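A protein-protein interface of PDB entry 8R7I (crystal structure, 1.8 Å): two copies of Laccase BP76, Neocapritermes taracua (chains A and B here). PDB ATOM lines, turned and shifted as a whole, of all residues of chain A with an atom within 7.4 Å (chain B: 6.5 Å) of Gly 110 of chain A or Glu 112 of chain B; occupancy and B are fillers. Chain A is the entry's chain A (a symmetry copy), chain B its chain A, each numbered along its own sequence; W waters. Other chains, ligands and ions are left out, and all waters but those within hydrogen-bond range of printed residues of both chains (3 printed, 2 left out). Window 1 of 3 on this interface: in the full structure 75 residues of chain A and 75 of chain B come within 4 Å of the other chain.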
ATOM      1  N   ASP A  47      -2.856 -19.557   2.908  1.00  0.00           N
ATOM      2  CA  ASP A  47      -1.798 -19.915   1.963  1.00  0.00           C
ATOM      3  C   ASP A  47      -2.047 -19.088   0.698  1.00  0.00           C
ATOM      4  O   ASP A  47      -3.158 -19.130   0.184  1.00  0.00           O
ATOM      5  CB  ASP A  47      -1.835 -21.417   1.652  1.00  0.00           C
ATOM      6  CG  ASP A  47      -1.703 -22.277   2.901  1.00  0.00           C
ATOM      7  OD1 ASP A  47      -0.668 -22.119   3.588  1.00  0.00           O
ATOM      8  OD2 ASP A  47      -2.656 -22.996   3.210  1.00  0.00           O
ATOM      9  N   ARG A  81       2.280 -16.569   3.166  1.00  0.00           N
ATOM     10  CA  ARG A  81       1.184 -16.624   4.143  1.00  0.00           C
ATOM     11  C   ARG A  81       0.727 -15.179   4.324  1.00  0.00           C
ATOM     12  O   ARG A  81       1.580 -14.335   4.600  1.00  0.00           O
ATOM     13  CB  ARG A  81       1.654 -17.240   5.467  1.00  0.00           C
ATOM     14  CG  ARG A  81       1.993 -18.723   5.357  1.00  0.00           C
ATOM     15  CD  ARG A  81       2.597 -19.298   6.641  1.00  0.00           C
ATOM     16  NE  ARG A  81       3.189 -20.581   6.280  1.00  0.00           N
ATOM     17  CZ  ARG A  81       2.486 -21.653   6.006  1.00  0.00           C
ATOM     18  NH1 ARG A  81       1.183 -21.631   6.193  1.00  0.00           N
ATOM     19  NH2 ARG A  81       3.066 -22.755   5.581  1.00  0.00           N
ATOM     20  N   ASN A 106      -8.056 -18.786  11.003  1.00  0.00           N
ATOM     21  CA  ASN A 106      -6.934 -19.600  10.528  1.00  0.00           C
ATOM     22  C   ASN A 106      -7.393 -20.515   9.382  1.00  0.00           C
ATOM     23  O   ASN A 106      -8.099 -21.466   9.643  1.00  0.00           O
ATOM     24  CB  ASN A 106      -6.282 -20.408  11.658  1.00  0.00           C
ATOM     25  CG  ASN A 106      -5.092 -21.196  11.171  1.00  0.00           C
ATOM     26  OD1 ASN A 106      -4.708 -21.062   9.992  1.00  0.00           O
ATOM     27  ND2 ASN A 106      -4.542 -22.046  12.022  1.00  0.00           N
ATOM     28  N   LYS A 107      -6.991 -20.226   8.148  1.00  0.00           N
ATOM     29  CA  LYS A 107      -7.325 -21.030   6.956  1.00  0.00           C
ATOM     30  C   LYS A 107      -6.054 -21.610   6.342  1.00  0.00           C
ATOM     31  O   LYS A 107      -6.026 -21.937   5.139  1.00  0.00           O
ATOM     32  CB  LYS A 107      -8.149 -20.141   6.028  1.00  0.00           C
ATOM     33  CG  LYS A 107      -8.720 -20.790   4.790  1.00  0.00           C
ATOM     34  CD  LYS A 107      -9.749 -21.873   5.051  1.00  0.00           C
ATOM     35  CE  LYS A 107     -10.352 -22.436   3.764  1.00  0.00           C
ATOM     36  NZ  LYS A 107     -11.164 -23.658   4.050  1.00  0.00           N
ATOM     37  N   MET A 108      -4.947 -21.706   7.128  1.00  0.00           N
ATOM     38  CA  MET A 108      -3.686 -22.209   6.579  1.00  0.00           C
ATOM     39  C   MET A 108      -3.586 -23.724   6.797  1.00  0.00           C
ATOM     40  O   MET A 108      -3.591 -24.188   7.950  1.00  0.00           O
ATOM     41  CB  MET A 108      -2.476 -21.515   7.222  1.00  0.00           C
ATOM     42  CG  MET A 108      -2.479 -20.000   6.933  1.00  0.00           C
ATOM     43  SD  MET A 108      -1.063 -19.143   7.634  1.00  0.00           S
ATOM     44  CE  MET A 108      -1.320 -19.428   9.368  1.00  0.00           C
ATOM     45  N   ALA A 109      -3.434 -24.466   5.694  1.00  0.00           N
ATOM     46  CA  ALA A 109      -3.421 -25.940   5.700  1.00  0.00           C
ATOM     47  C   ALA A 109      -2.343 -26.446   6.670  1.00  0.00           C
ATOM     48  O   ALA A 109      -1.165 -26.089   6.508  1.00  0.00           O
ATOM     49  CB  ALA A 109      -3.088 -26.397   4.279  1.00  0.00           C
ATOM     50  N   GLY A 110      -2.697 -27.267   7.649  1.00  0.00           N
ATOM     51  CA  GLY A 110      -1.710 -27.913   8.493  1.00  0.00           C
ATOM     52  C   GLY A 110      -1.012 -26.993   9.491  1.00  0.00           C
ATOM     53  O   GLY A 110      -0.088 -27.452  10.191  1.00  0.00           O
ATOM     54  N   ASN A 111      -1.376 -25.703   9.528  1.00  0.00           N
ATOM     55  CA  ASN A 111      -0.675 -24.709  10.369  1.00  0.00           C
ATOM     56  C   ASN A 111      -1.548 -24.296  11.555  1.00  0.00           C
ATOM     57  O   ASN A 111      -2.778 -24.262  11.475  1.00  0.00           O
ATOM     58  CB  ASN A 111      -0.233 -23.476   9.567  1.00  0.00           C
ATOM     59  CG  ASN A 111       1.116 -23.661   8.905  1.00  0.00           C
ATOM     60  OD1 ASN A 111       2.044 -22.895   9.139  1.00  0.00           O
ATOM     61  ND2 ASN A 111       1.293 -24.726   8.169  1.00  0.00           N
ATOM     62  N   GLU A 112      -0.911 -24.045  12.704  1.00  0.00           N
ATOM     63  CA  GLU A 112      -1.553 -23.389  13.836  1.00  0.00           C
ATOM     64  C   GLU A 112      -1.175 -21.895  13.770  1.00  0.00           C
ATOM     65  O   GLU A 112      -0.187 -21.537  13.077  1.00  0.00           O
ATOM     66  CB  GLU A 112      -1.101 -24.027  15.156  1.00  0.00           C
ATOM     67  CG  GLU A 112       0.405 -23.997  15.352  1.00  0.00           C
ATOM     68  CD  GLU A 112       0.913 -24.570  16.662  1.00  0.00           C
ATOM     69  OE1 GLU A 112       0.446 -25.622  17.055  1.00  0.00           O
ATOM     70  OE2 GLU A 112       1.840 -23.962  17.240  1.00  0.00           O
ATOM     71  N   LEU A 113      -1.926 -21.036  14.459  1.00  0.00           N
ATOM     72  CA  LEU A 113      -1.720 -19.587  14.353  1.00  0.00           C
ATOM     73  C   LEU A 113      -1.904 -18.867  15.684  1.00  0.00           C
ATOM     74  O   LEU A 113      -2.801 -19.195  16.476  1.00  0.00           O
ATOM     75  CB  LEU A 113      -2.683 -19.039  13.297  1.00  0.00           C
ATOM     76  CG  LEU A 113      -2.678 -17.523  13.044  1.00  0.00           C
ATOM     77  CD1 LEU A 113      -1.345 -17.007  12.497  1.00  0.00           C
ATOM     78  CD2 LEU A 113      -3.785 -17.182  12.068  1.00  0.00           C
ATOM     79  N   SER A 138      -2.464 -21.972  20.606  1.00  0.00           N
ATOM     80  CA  SER A 138      -2.533 -21.614  19.194  1.00  0.00           C
ATOM     81  C   SER A 138      -3.930 -21.939  18.634  1.00  0.00           C
ATOM     82  O   SER A 138      -4.572 -22.919  19.062  1.00  0.00           O
ATOM     83  CB  SER A 138      -1.464 -22.301  18.382  1.00  0.00           C
ATOM     84  OG  SER A 138      -0.177 -21.940  18.843  1.00  0.00           O
ATOM     85  N   ILE A 139      -4.286 -21.213  17.571  1.00  0.00           N
ATOM     86  CA  ILE A 139      -5.551 -21.367  16.851  1.00  0.00           C
ATOM     87  C   ILE A 139      -5.374 -22.478  15.826  1.00  0.00           C
ATOM     88  O   ILE A 139      -4.516 -22.333  14.917  1.00  0.00           O
ATOM     89  CB  ILE A 139      -5.949 -20.035  16.171  1.00  0.00           C
ATOM     90  CG1 ILE A 139      -5.865 -18.844  17.120  1.00  0.00           C
ATOM     91  CG2 ILE A 139      -7.321 -20.140  15.500  1.00  0.00           C
ATOM     92  CD1 ILE A 139      -5.752 -17.523  16.412  1.00  0.00           C
ATOM     93  N   LEU A 140      -6.231 -23.510  15.906  1.00  0.00           N
ATOM     94  CA  LEU A 140      -6.199 -24.602  14.957  1.00  0.00           C
ATOM     95  C   LEU A 140      -6.784 -24.155  13.609  1.00  0.00           C
ATOM     96  O   LEU A 140      -7.619 -23.250  13.562  1.00  0.00           O
ATOM     97  CB  LEU A 140      -6.973 -25.804  15.510  1.00  0.00           C
ATOM     98  CG  LEU A 140      -6.400 -26.364  16.815  1.00  0.00           C
ATOM     99  CD1 LEU A 140      -7.274 -27.457  17.338  1.00  0.00           C
ATOM    100  CD2 LEU A 140      -4.976 -26.889  16.569  1.00  0.00           C
ATOM    101  N   GLU A 141      -6.350 -24.818  12.543  1.00  0.00           N
ATOM    102  CA  GLU A 141      -6.886 -24.551  11.222  1.00  0.00           C
ATOM    103  C   GLU A 141      -8.395 -24.864  11.262  1.00  0.00           C
ATOM    104  O   GLU A 141      -8.761 -25.899  11.809  1.00  0.00           O
ATOM    105  CB  GLU A 141      -6.188 -25.396  10.175  1.00  0.00           C
ATOM    106  CG  GLU A 141      -6.443 -24.923   8.751  1.00  0.00           C
ATOM    107  CD  GLU A 141      -7.816 -25.273   8.238  1.00  0.00           C
ATOM    108  OE1 GLU A 141      -8.399 -26.263   8.721  1.00  0.00           O
ATOM    109  OE2 GLU A 141      -8.344 -24.531   7.318  1.00  0.00           O
ATOM    110  N   GLY A 142      -9.216 -23.941  10.758  1.00  0.00           N
ATOM    111  CA  GLY A 142     -10.677 -24.082  10.743  1.00  0.00           C
ATOM    112  C   GLY A 142     -11.340 -23.337  11.890  1.00  0.00           C
ATOM    113  O   GLY A 142     -12.584 -23.250  11.901  1.00  0.00           O
ATOM    114  N   ASP A 163       3.957 -17.731  15.790  1.00  0.00           N
ATOM    115  CA  ASP A 163       3.779 -19.188  15.684  1.00  0.00           C
ATOM    116  C   ASP A 163       4.712 -19.694  14.588  1.00  0.00           C
ATOM    117  O   ASP A 163       4.454 -19.443  13.401  1.00  0.00           O
ATOM    118  CB  ASP A 163       2.315 -19.549  15.441  1.00  0.00           C
ATOM    119  CG  ASP A 163       1.867 -20.817  16.130  1.00  0.00           C
ATOM    120  OD1 ASP A 163       2.707 -21.763  16.240  1.00  0.00           O
ATOM    121  OD2 ASP A 163       0.676 -20.841  16.585  1.00  0.00           O
ATOM    122  N   GLN A 166       6.168 -18.168  10.401  1.00  0.00           N
ATOM    123  CA  GLN A 166       5.145 -17.590   9.513  1.00  0.00           C
ATOM    124  C   GLN A 166       5.354 -16.077   9.252  1.00  0.00           C
ATOM    125  O   GLN A 166       4.935 -15.585   8.189  1.00  0.00           O
ATOM    126  CB  GLN A 166       3.755 -17.813  10.154  1.00  0.00           C
ATOM    127  CG  GLN A 166       3.383 -19.291  10.286  1.00  0.00           C
ATOM    128  CD  GLN A 166       2.183 -19.479  11.205  1.00  0.00           C
ATOM    129  OE1 GLN A 166       1.659 -18.530  11.788  1.00  0.00           O
ATOM    130  NE2 GLN A 166       1.783 -20.724  11.354  1.00  0.00           N
ATOM    131  N   ASN B 106       4.649 -33.629  18.583  1.00  0.00           N
ATOM    132  CA  ASN B 106       4.679 -32.608  17.532  1.00  0.00           C
ATOM    133  C   ASN B 106       5.778 -31.577  17.831  1.00  0.00           C
ATOM    134  O   ASN B 106       5.606 -30.784  18.732  1.00  0.00           O
ATOM    135  CB  ASN B 106       3.317 -31.928  17.343  1.00  0.00           C
ATOM    136  CG  ASN B 106       3.343 -30.921  16.221  1.00  0.00           C
ATOM    137  OD1 ASN B 106       4.372 -30.800  15.528  1.00  0.00           O
ATOM    138  ND2 ASN B 106       2.268 -30.164  16.062  1.00  0.00           N
ATOM    139  N   MET B 108       7.080 -29.710  15.128  1.00  0.00           N
ATOM    140  CA  MET B 108       7.182 -28.961  13.874  1.00  0.00           C
ATOM    141  C   MET B 108       6.750 -27.506  14.095  1.00  0.00           C
ATOM    142  O   MET B 108       5.594 -27.251  14.476  1.00  0.00           O
ATOM    143  CB  MET B 108       6.320 -29.592  12.770  1.00  0.00           C
ATOM    144  CG  MET B 108       6.792 -31.023  12.438  1.00  0.00           C
ATOM    145  SD  MET B 108       5.838 -31.796  11.126  1.00  0.00           S
ATOM    146  CE  MET B 108       4.225 -31.849  11.866  1.00  0.00           C
ATOM    147  N   GLY B 110       5.230 -24.077  14.076  1.00  0.00           N
ATOM    148  CA  GLY B 110       4.066 -23.463  13.467  1.00  0.00           C
ATOM    149  C   GLY B 110       3.041 -24.442  12.902  1.00  0.00           C
ATOM    150  O   GLY B 110       2.055 -23.994  12.283  1.00  0.00           O
ATOM    151  N   ASN B 111       3.275 -25.755  13.036  1.00  0.00           N
ATOM    152  CA  ASN B 111       2.407 -26.779  12.416  1.00  0.00           C
ATOM    153  C   ASN B 111       1.578 -27.500  13.482  1.00  0.00           C
ATOM    154  O   ASN B 111       2.004 -27.679  14.624  1.00  0.00           O
ATOM    155  CB  ASN B 111       3.205 -27.789  11.577  1.00  0.00           C
ATOM    156  CG  ASN B 111       3.431 -27.320  10.156  1.00  0.00           C
ATOM    157  OD1 ASN B 111       3.048 -27.987   9.203  1.00  0.00           O
ATOM    158  ND2 ASN B 111       3.944 -26.130   9.981  1.00  0.00           N
ATOM    159  N   GLU B 112       0.340 -27.859  13.129  1.00  0.00           N
ATOM    160  CA  GLU B 112      -0.471 -28.777  13.919  1.00  0.00           C
ATOM    161  C   GLU B 112      -0.321 -30.176  13.287  1.00  0.00           C
ATOM    162  O   GLU B 112       0.107 -30.278  12.107  1.00  0.00           O
ATOM    163  CB  GLU B 112      -1.936 -28.322  13.938  1.00  0.00           C
ATOM    164  CG  GLU B 112      -2.543 -28.189  12.553  1.00  0.00           C
ATOM    165  CD  GLU B 112      -4.006 -27.789  12.506  1.00  0.00           C
ATOM    166  OE1 GLU B 112      -4.384 -26.889  13.232  1.00  0.00           O
ATOM    167  OE2 GLU B 112      -4.737 -28.361  11.669  1.00  0.00           O
ATOM    168  N   LEU B 113      -0.653 -31.230  14.030  1.00  0.00           N
ATOM    169  CA  LEU B 113      -0.423 -32.600  13.559  1.00  0.00           C
ATOM    170  C   LEU B 113      -1.544 -33.556  13.954  1.00  0.00           C
ATOM    171  O   LEU B 113      -2.087 -33.488  15.067  1.00  0.00           O
ATOM    172  CB  LEU B 113       0.923 -33.080  14.109  1.00  0.00           C
ATOM    173  CG  LEU B 113       1.359 -34.515  13.779  1.00  0.00           C
ATOM    174  CD1 LEU B 113       1.570 -34.753  12.282  1.00  0.00           C
ATOM    175  CD2 LEU B 113       2.642 -34.825  14.521  1.00  0.00           C
ATOM    176  N   ALA B 114      -1.838 -34.494  13.052  1.00  0.00           N
ATOM    177  CA  ALA B 114      -2.651 -35.669  13.372  1.00  0.00           C
ATOM    178  C   ALA B 114      -2.247 -36.757  12.378  1.00  0.00           C
ATOM    179  O   ALA B 114      -2.010 -36.437  11.209  1.00  0.00           O
ATOM    180  CB  ALA B 114      -4.126 -35.364  13.267  1.00  0.00           C
ATOM    181  N   PRO B 132      -8.359 -34.310  11.786  1.00  0.00           N
ATOM    182  CA  PRO B 132      -8.594 -32.976  12.353  1.00  0.00           C
ATOM    183  C   PRO B 132     -10.024 -32.491  12.111  1.00  0.00           C
ATOM    184  O   PRO B 132     -10.533 -32.621  10.999  1.00  0.00           O
ATOM    185  CB  PRO B 132      -7.619 -32.058  11.579  1.00  0.00           C
ATOM    186  CG  PRO B 132      -6.492 -33.009  11.171  1.00  0.00           C
ATOM    187  CD  PRO B 132      -7.208 -34.287  10.841  1.00  0.00           C
ATOM    188  N   MET B 133     -10.669 -31.998  13.169  1.00  0.00           N
ATOM    189  CA  MET B 133     -12.043 -31.466  13.142  1.00  0.00           C
ATOM    190  C   MET B 133     -13.057 -32.520  12.679  1.00  0.00           C
ATOM    191  O   MET B 133     -14.146 -32.131  12.238  1.00  0.00           O
ATOM    192  CB  MET B 133     -12.154 -30.186  12.298  1.00  0.00           C
ATOM    193  CG  MET B 133     -11.201 -29.091  12.753  1.00  0.00           C
ATOM    194  SD  MET B 133     -11.381 -28.787  14.549  1.00  0.00           S
ATOM    195  CE  MET B 133     -10.615 -27.164  14.635  1.00  0.00           C
ATOM    196  N   SER B 138      -6.468 -31.440  16.288  1.00  0.00           N
ATOM    197  CA  SER B 138      -5.060 -31.556  15.928  1.00  0.00           C
ATOM    198  C   SER B 138      -4.177 -31.324  17.168  1.00  0.00           C
ATOM    199  O   SER B 138      -4.531 -30.524  18.057  1.00  0.00           O
ATOM    200  CB  SER B 138      -4.678 -30.608  14.820  1.00  0.00           C
ATOM    201  OG  SER B 138      -5.431 -30.873  13.653  1.00  0.00           O
ATOM    202  N   ILE B 139      -2.973 -31.897  17.107  1.00  0.00           N
ATOM    203  CA  ILE B 139      -1.952 -31.787  18.152  1.00  0.00           C
ATOM    204  C   ILE B 139      -1.171 -30.504  17.910  1.00  0.00           C
ATOM    205  O   ILE B 139      -0.529 -30.378  16.834  1.00  0.00           O
ATOM    206  CB  ILE B 139      -1.021 -33.023  18.126  1.00  0.00           C
ATOM    207  CG1 ILE B 139      -1.792 -34.338  18.087  1.00  0.00           C
ATOM    208  CG2 ILE B 139      -0.010 -32.983  19.276  1.00  0.00           C
ATOM    209  CD1 ILE B 139      -0.979 -35.492  17.569  1.00  0.00           C
ATOM    210  N   LEU B 140      -1.139 -29.620  18.922  1.00  0.00           N
ATOM    211  CA  LEU B 140      -0.388 -28.387  18.834  1.00  0.00           C
ATOM    212  C   LEU B 140       1.117 -28.668  18.966  1.00  0.00           C
ATOM    213  O   LEU B 140       1.513 -29.652  19.592  1.00  0.00           O
ATOM    214  CB  LEU B 140      -0.852 -27.408  19.918  1.00  0.00           C
ATOM    215  CG  LEU B 140      -2.326 -27.011  19.806  1.00  0.00           C
ATOM    216  CD1 LEU B 140      -2.720 -26.146  20.959  1.00  0.00           C
ATOM    217  CD2 LEU B 140      -2.561 -26.271  18.479  1.00  0.00           C
ATOM    218  N   GLU B 141       1.922 -27.781  18.391  1.00  0.00           N
ATOM    219  CA  GLU B 141       3.364 -27.885  18.515  1.00  0.00           C
ATOM    220  C   GLU B 141       3.709 -27.783  20.015  1.00  0.00           C
ATOM    221  O   GLU B 141       3.157 -26.913  20.681  1.00  0.00           O
ATOM    222  CB  GLU B 141       4.052 -26.790  17.726  1.00  0.00           C
ATOM    223  CG  GLU B 141       5.541 -27.041  17.521  1.00  0.00           C
ATOM    224  CD  GLU B 141       6.368 -26.789  18.754  1.00  0.00           C
ATOM    225  OE1 GLU B 141       5.945 -25.981  19.602  1.00  0.00           O
ATOM    226  OE2 GLU B 141       7.489 -27.425  18.890  1.00  0.00           O
ATOM    227  N   SER B 161       0.214 -38.364   7.913  1.00  0.00           N
ATOM    228  CA  SER B 161      -0.390 -37.139   8.403  1.00  0.00           C
ATOM    229  C   SER B 161      -1.700 -36.919   7.660  1.00  0.00           C
ATOM    230  O   SER B 161      -1.731 -37.072   6.417  1.00  0.00           O
ATOM    231  CB  SER B 161       0.503 -35.946   8.240  1.00  0.00           C
ATOM    232  OG  SER B 161      -0.252 -34.800   8.545  1.00  0.00           O
ATOM    233  N   ASP B 163      -3.146 -33.923   8.214  1.00  0.00           N
ATOM    234  CA  ASP B 163      -3.184 -32.505   8.606  1.00  0.00           C
ATOM    235  C   ASP B 163      -2.469 -31.702   7.522  1.00  0.00           C
ATOM    236  O   ASP B 163      -1.236 -31.777   7.418  1.00  0.00           O
ATOM    237  CB  ASP B 163      -2.587 -32.301   9.996  1.00  0.00           C
ATOM    238  CG  ASP B 163      -3.282 -31.239  10.818  1.00  0.00           C
ATOM    239  OD1 ASP B 163      -3.744 -30.225  10.209  1.00  0.00           O
ATOM    240  OD2 ASP B 163      -3.382 -31.448  12.072  1.00  0.00           O
ATOM    241  N   GLY B 164      -3.241 -31.023   6.664  1.00  0.00           N
ATOM    242  CA  GLY B 164      -2.680 -30.240   5.560  1.00  0.00           C
ATOM    243  C   GLY B 164      -1.910 -31.143   4.595  1.00  0.00           C
ATOM    244  O   GLY B 164      -2.374 -32.246   4.281  1.00  0.00           O
ATOM    245  N   LEU B 165      -0.739 -30.672   4.139  1.00  0.00           N
ATOM    246  CA  LEU B 165      -0.006 -31.244   3.013  1.00  0.00           C
ATOM    247  C   LEU B 165       1.226 -32.010   3.488  1.00  0.00           C
ATOM    248  O   LEU B 165       2.108 -32.317   2.689  1.00  0.00           O
ATOM    249  CB  LEU B 165       0.376 -30.094   2.087  1.00  0.00           C
ATOM    250  CG  LEU B 165      -0.796 -29.173   1.704  1.00  0.00           C
ATOM    251  CD1 LEU B 165      -0.231 -27.964   0.968  1.00  0.00           C
ATOM    252  CD2 LEU B 165      -1.815 -29.927   0.843  1.00  0.00           C
ATOM    253  N   GLN B 166       1.300 -32.286   4.796  1.00  0.00           N
ATOM    254  CA  GLN B 166       2.507 -32.831   5.442  1.00  0.00           C
ATOM    255  C   GLN B 166       2.892 -34.237   4.916  1.00  0.00           C
ATOM    256  O   GLN B 166       4.085 -34.589   4.956  1.00  0.00           O
ATOM    257  CB  GLN B 166       2.260 -32.903   6.966  1.00  0.00           C
ATOM    258  CG  GLN B 166       2.047 -31.530   7.607  1.00  0.00           C
ATOM    259  CD  GLN B 166       1.486 -31.660   9.018  1.00  0.00           C
ATOM    260  OE1 GLN B 166       1.202 -32.755   9.503  1.00  0.00           O
ATOM    261  NE2 GLN B 166       1.296 -30.521   9.651  1.00  0.00           N
HETATM  262  O   HOH W   1      -7.511 -28.354  12.472  1.00  0.00           O
HETATM  263  O   HOH W   2       0.392 -28.265   5.314  1.00  0.00           O
HETATM  264  O   HOH W   3       1.858 -24.467  20.084  1.00  0.00           O
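Of chain B, only Asn 111, Glu 112, Asp 163, Gly 164 and Gln 166 come within 4 Å of Gly 110 of chain A.
Of the printed residues of chain A, Glu 112 of chain B touches Gly 110, Asn 111, Leu 140 and Glu 141.
Of the printed residues of chain B, Glu 141 of chain A touches Glu 112 (2.9 Å) and Met 133 (3.6 Å).
Of the printed residues of chain A, Met 133 of chain B touches Leu 140 and Glu 141.
Of the printed residues of chain A, Leu 140 of chain B touches Glu 112, Ser 138 and Leu 140.
Of the printed residues of chain A, Gly 164 of chain B touches Ala 109 and Gly 110.
Printed residues of chain B within 4 Å of Gln 166 of chain A: Gly 110.
Met 108 of chain B touches none of the printed residues of chain A.
The nearest residue of chain A that does not touch Glu 112 of chain B is Glu 112 of chain A (4.04 Å).
Among the printed residues, pairs that only touch across the chains: Leu 140 of chain A with Leu 140 of chain B (3.1 Å), Leu 140 of chain A with Glu 112 of chain B (3.4 Å), Glu 112 of chain A with Leu 140 of chain B (3.4 Å), Asn 111 of chain A with Asn 111 of chain B (3.5 Å), Asp 163 of chain A with Gly 110 of chain B (3.5 Å), Gly 110 of chain A with Asp 163 of chain B (3.5 Å), Asn 111 of chain A with Glu 112 of chain B (3.5 Å), Glu 112 of chain A with Asn 111 of chain B (3.5 Å), Glu 141 of chain A with Met 133 of chain B (3.6 Å), Gly 110 of chain A with Gly 164 of chain B (3.6 Å), Ser 138 of chain A with Leu 140 of chain B (3.95 Å), Leu 140 of chain A with Ser 138 of chain B (3.95 Å), Ala 109 of chain A with Gly 164 of chain B (3.97 Å) and Leu 140 of chain A with Met 133 of chain B (3.98 Å).
Gly 110 of chain A touches Asn 111 of chain B, and with the chains exchanged Asn 111 of chain A touches Gly 110 of chain B.
Gly 110 of chain A touches Glu 112 of chain B, and with the chains exchanged Glu 112 of chain A touches Gly 110 of chain B.
Glu 112 of chain A touches Leu 140 of chain B, and with the chains exchanged Leu 140 of chain A touches Glu 112 of chain B.
Ser 138 of chain A touches Leu 140 of chain B, and with the chains exchanged Leu 140 of chain A touches Ser 138 of chain B.
Positions printed for both chains: 106, 108, 110, 111, 112, 113, 138, 139, 140, 141, 163 and 166.
Of the 22 pairs that touch across the chains among the printed residues, 18 have their exchanged pair printed and touching as well.
Of the 17 printed residues of chain A, 9 touch a printed residue of chain B.
Printed residues of chain A that touch a printed residue of chain B: Ala 109, Gly 110, Asn 111, Glu 112, Ser 138, Leu 140, Glu 141, Asp 163 and Gln 166.
Among the printed residues, no Asp or Glu carboxylate lies within 4 Å of a Lys or Arg side-chain nitrogen of the other chain.
Water W1 lies within hydrogen-bond range of O of Glu 141 of chain A (2.8 Å), OE2 of Glu 112 of chain B (2.9 Å) and OG of Ser 138 of chain B (3.5 Å).
Water W3 lies within hydrogen-bond range of the backbone carbonyl oxygen (O) of Glu 141 of chain B (2.8 Å), the side-chain carboxylate (OE2) of Glu 112 of chain A (2.9 Å) and the side-chain hydroxyl (OG) of Ser 138 of chain A (3.5 Å).
Water W2 lies within hydrogen-bond range of the backbone NH of Leu 165 of chain B (2.9 Å) and the backbone carbonyl oxygen of Ala 109 of chain A (2.9 Å).
The backbone carbonyl oxygen (O) of Gly 110 of chain B lies close to the side-chain amide oxygen (OD1) of Asn 111 of chain A, at 3.3 Å.
The backbone carbonyl oxygen (O) of Gly 110 of chain B sits at hydrogen-bond distance from the backbone NH (N) of Glu 112 of chain A.
The backbone carbonyl oxygen of Gly 110 of chain B is in hydrogen-bond range of the side-chain amide nitrogen of Gln 166 of chain A (3.4 Å).
OD1 of Asn 111 of chain B lies close to O of Gly 110 of chain A (3.3 Å).
The backbone NH of Glu 112 of chain B sits at hydrogen-bond distance from the backbone carbonyl oxygen of Gly 110 of chain A.
OE1 of Glu 112 of chain B sits at hydrogen-bond distance from N of Glu 141 of chain A (2.9 Å).
The backbone NH (N) of Glu 141 of chain B lies within hydrogen-bond range of the side-chain carboxylate (OE1) of Glu 112 of chain A.
NE2 of Gln 166 of chain B lies within hydrogen-bond range of O of Gly 110 of chain A (3.4 Å).
The side-chain amide nitrogen of Asn 106 of chain B sits at hydrogen-bond distance from the backbone carbonyl oxygen of Asn 111 of chain B (2.9 Å).
The side-chain carboxylate of Asp 47 of chain A lies within hydrogen-bond range of the backbone NH of Ala 109 of chain A.
NE2 of Gln 166 of chain A sits at hydrogen-bond distance from OD1 of Asn 111 of chain A, at 3.1 Å.
The side-chain carboxylate of Asp 163 of chain A sits close to the side-chain carboxylate of Glu 112 of chain A.
The side-chain carboxylate of Asp 163 of chain A is in hydrogen-bond range of the side-chain hydroxyl of Ser 138 of chain A, at 2.7 Å.
The backbone carbonyl oxygen of Asp 163 of chain A sits close to the side-chain amide oxygen of Gln 166 of chain A (3.4 Å).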
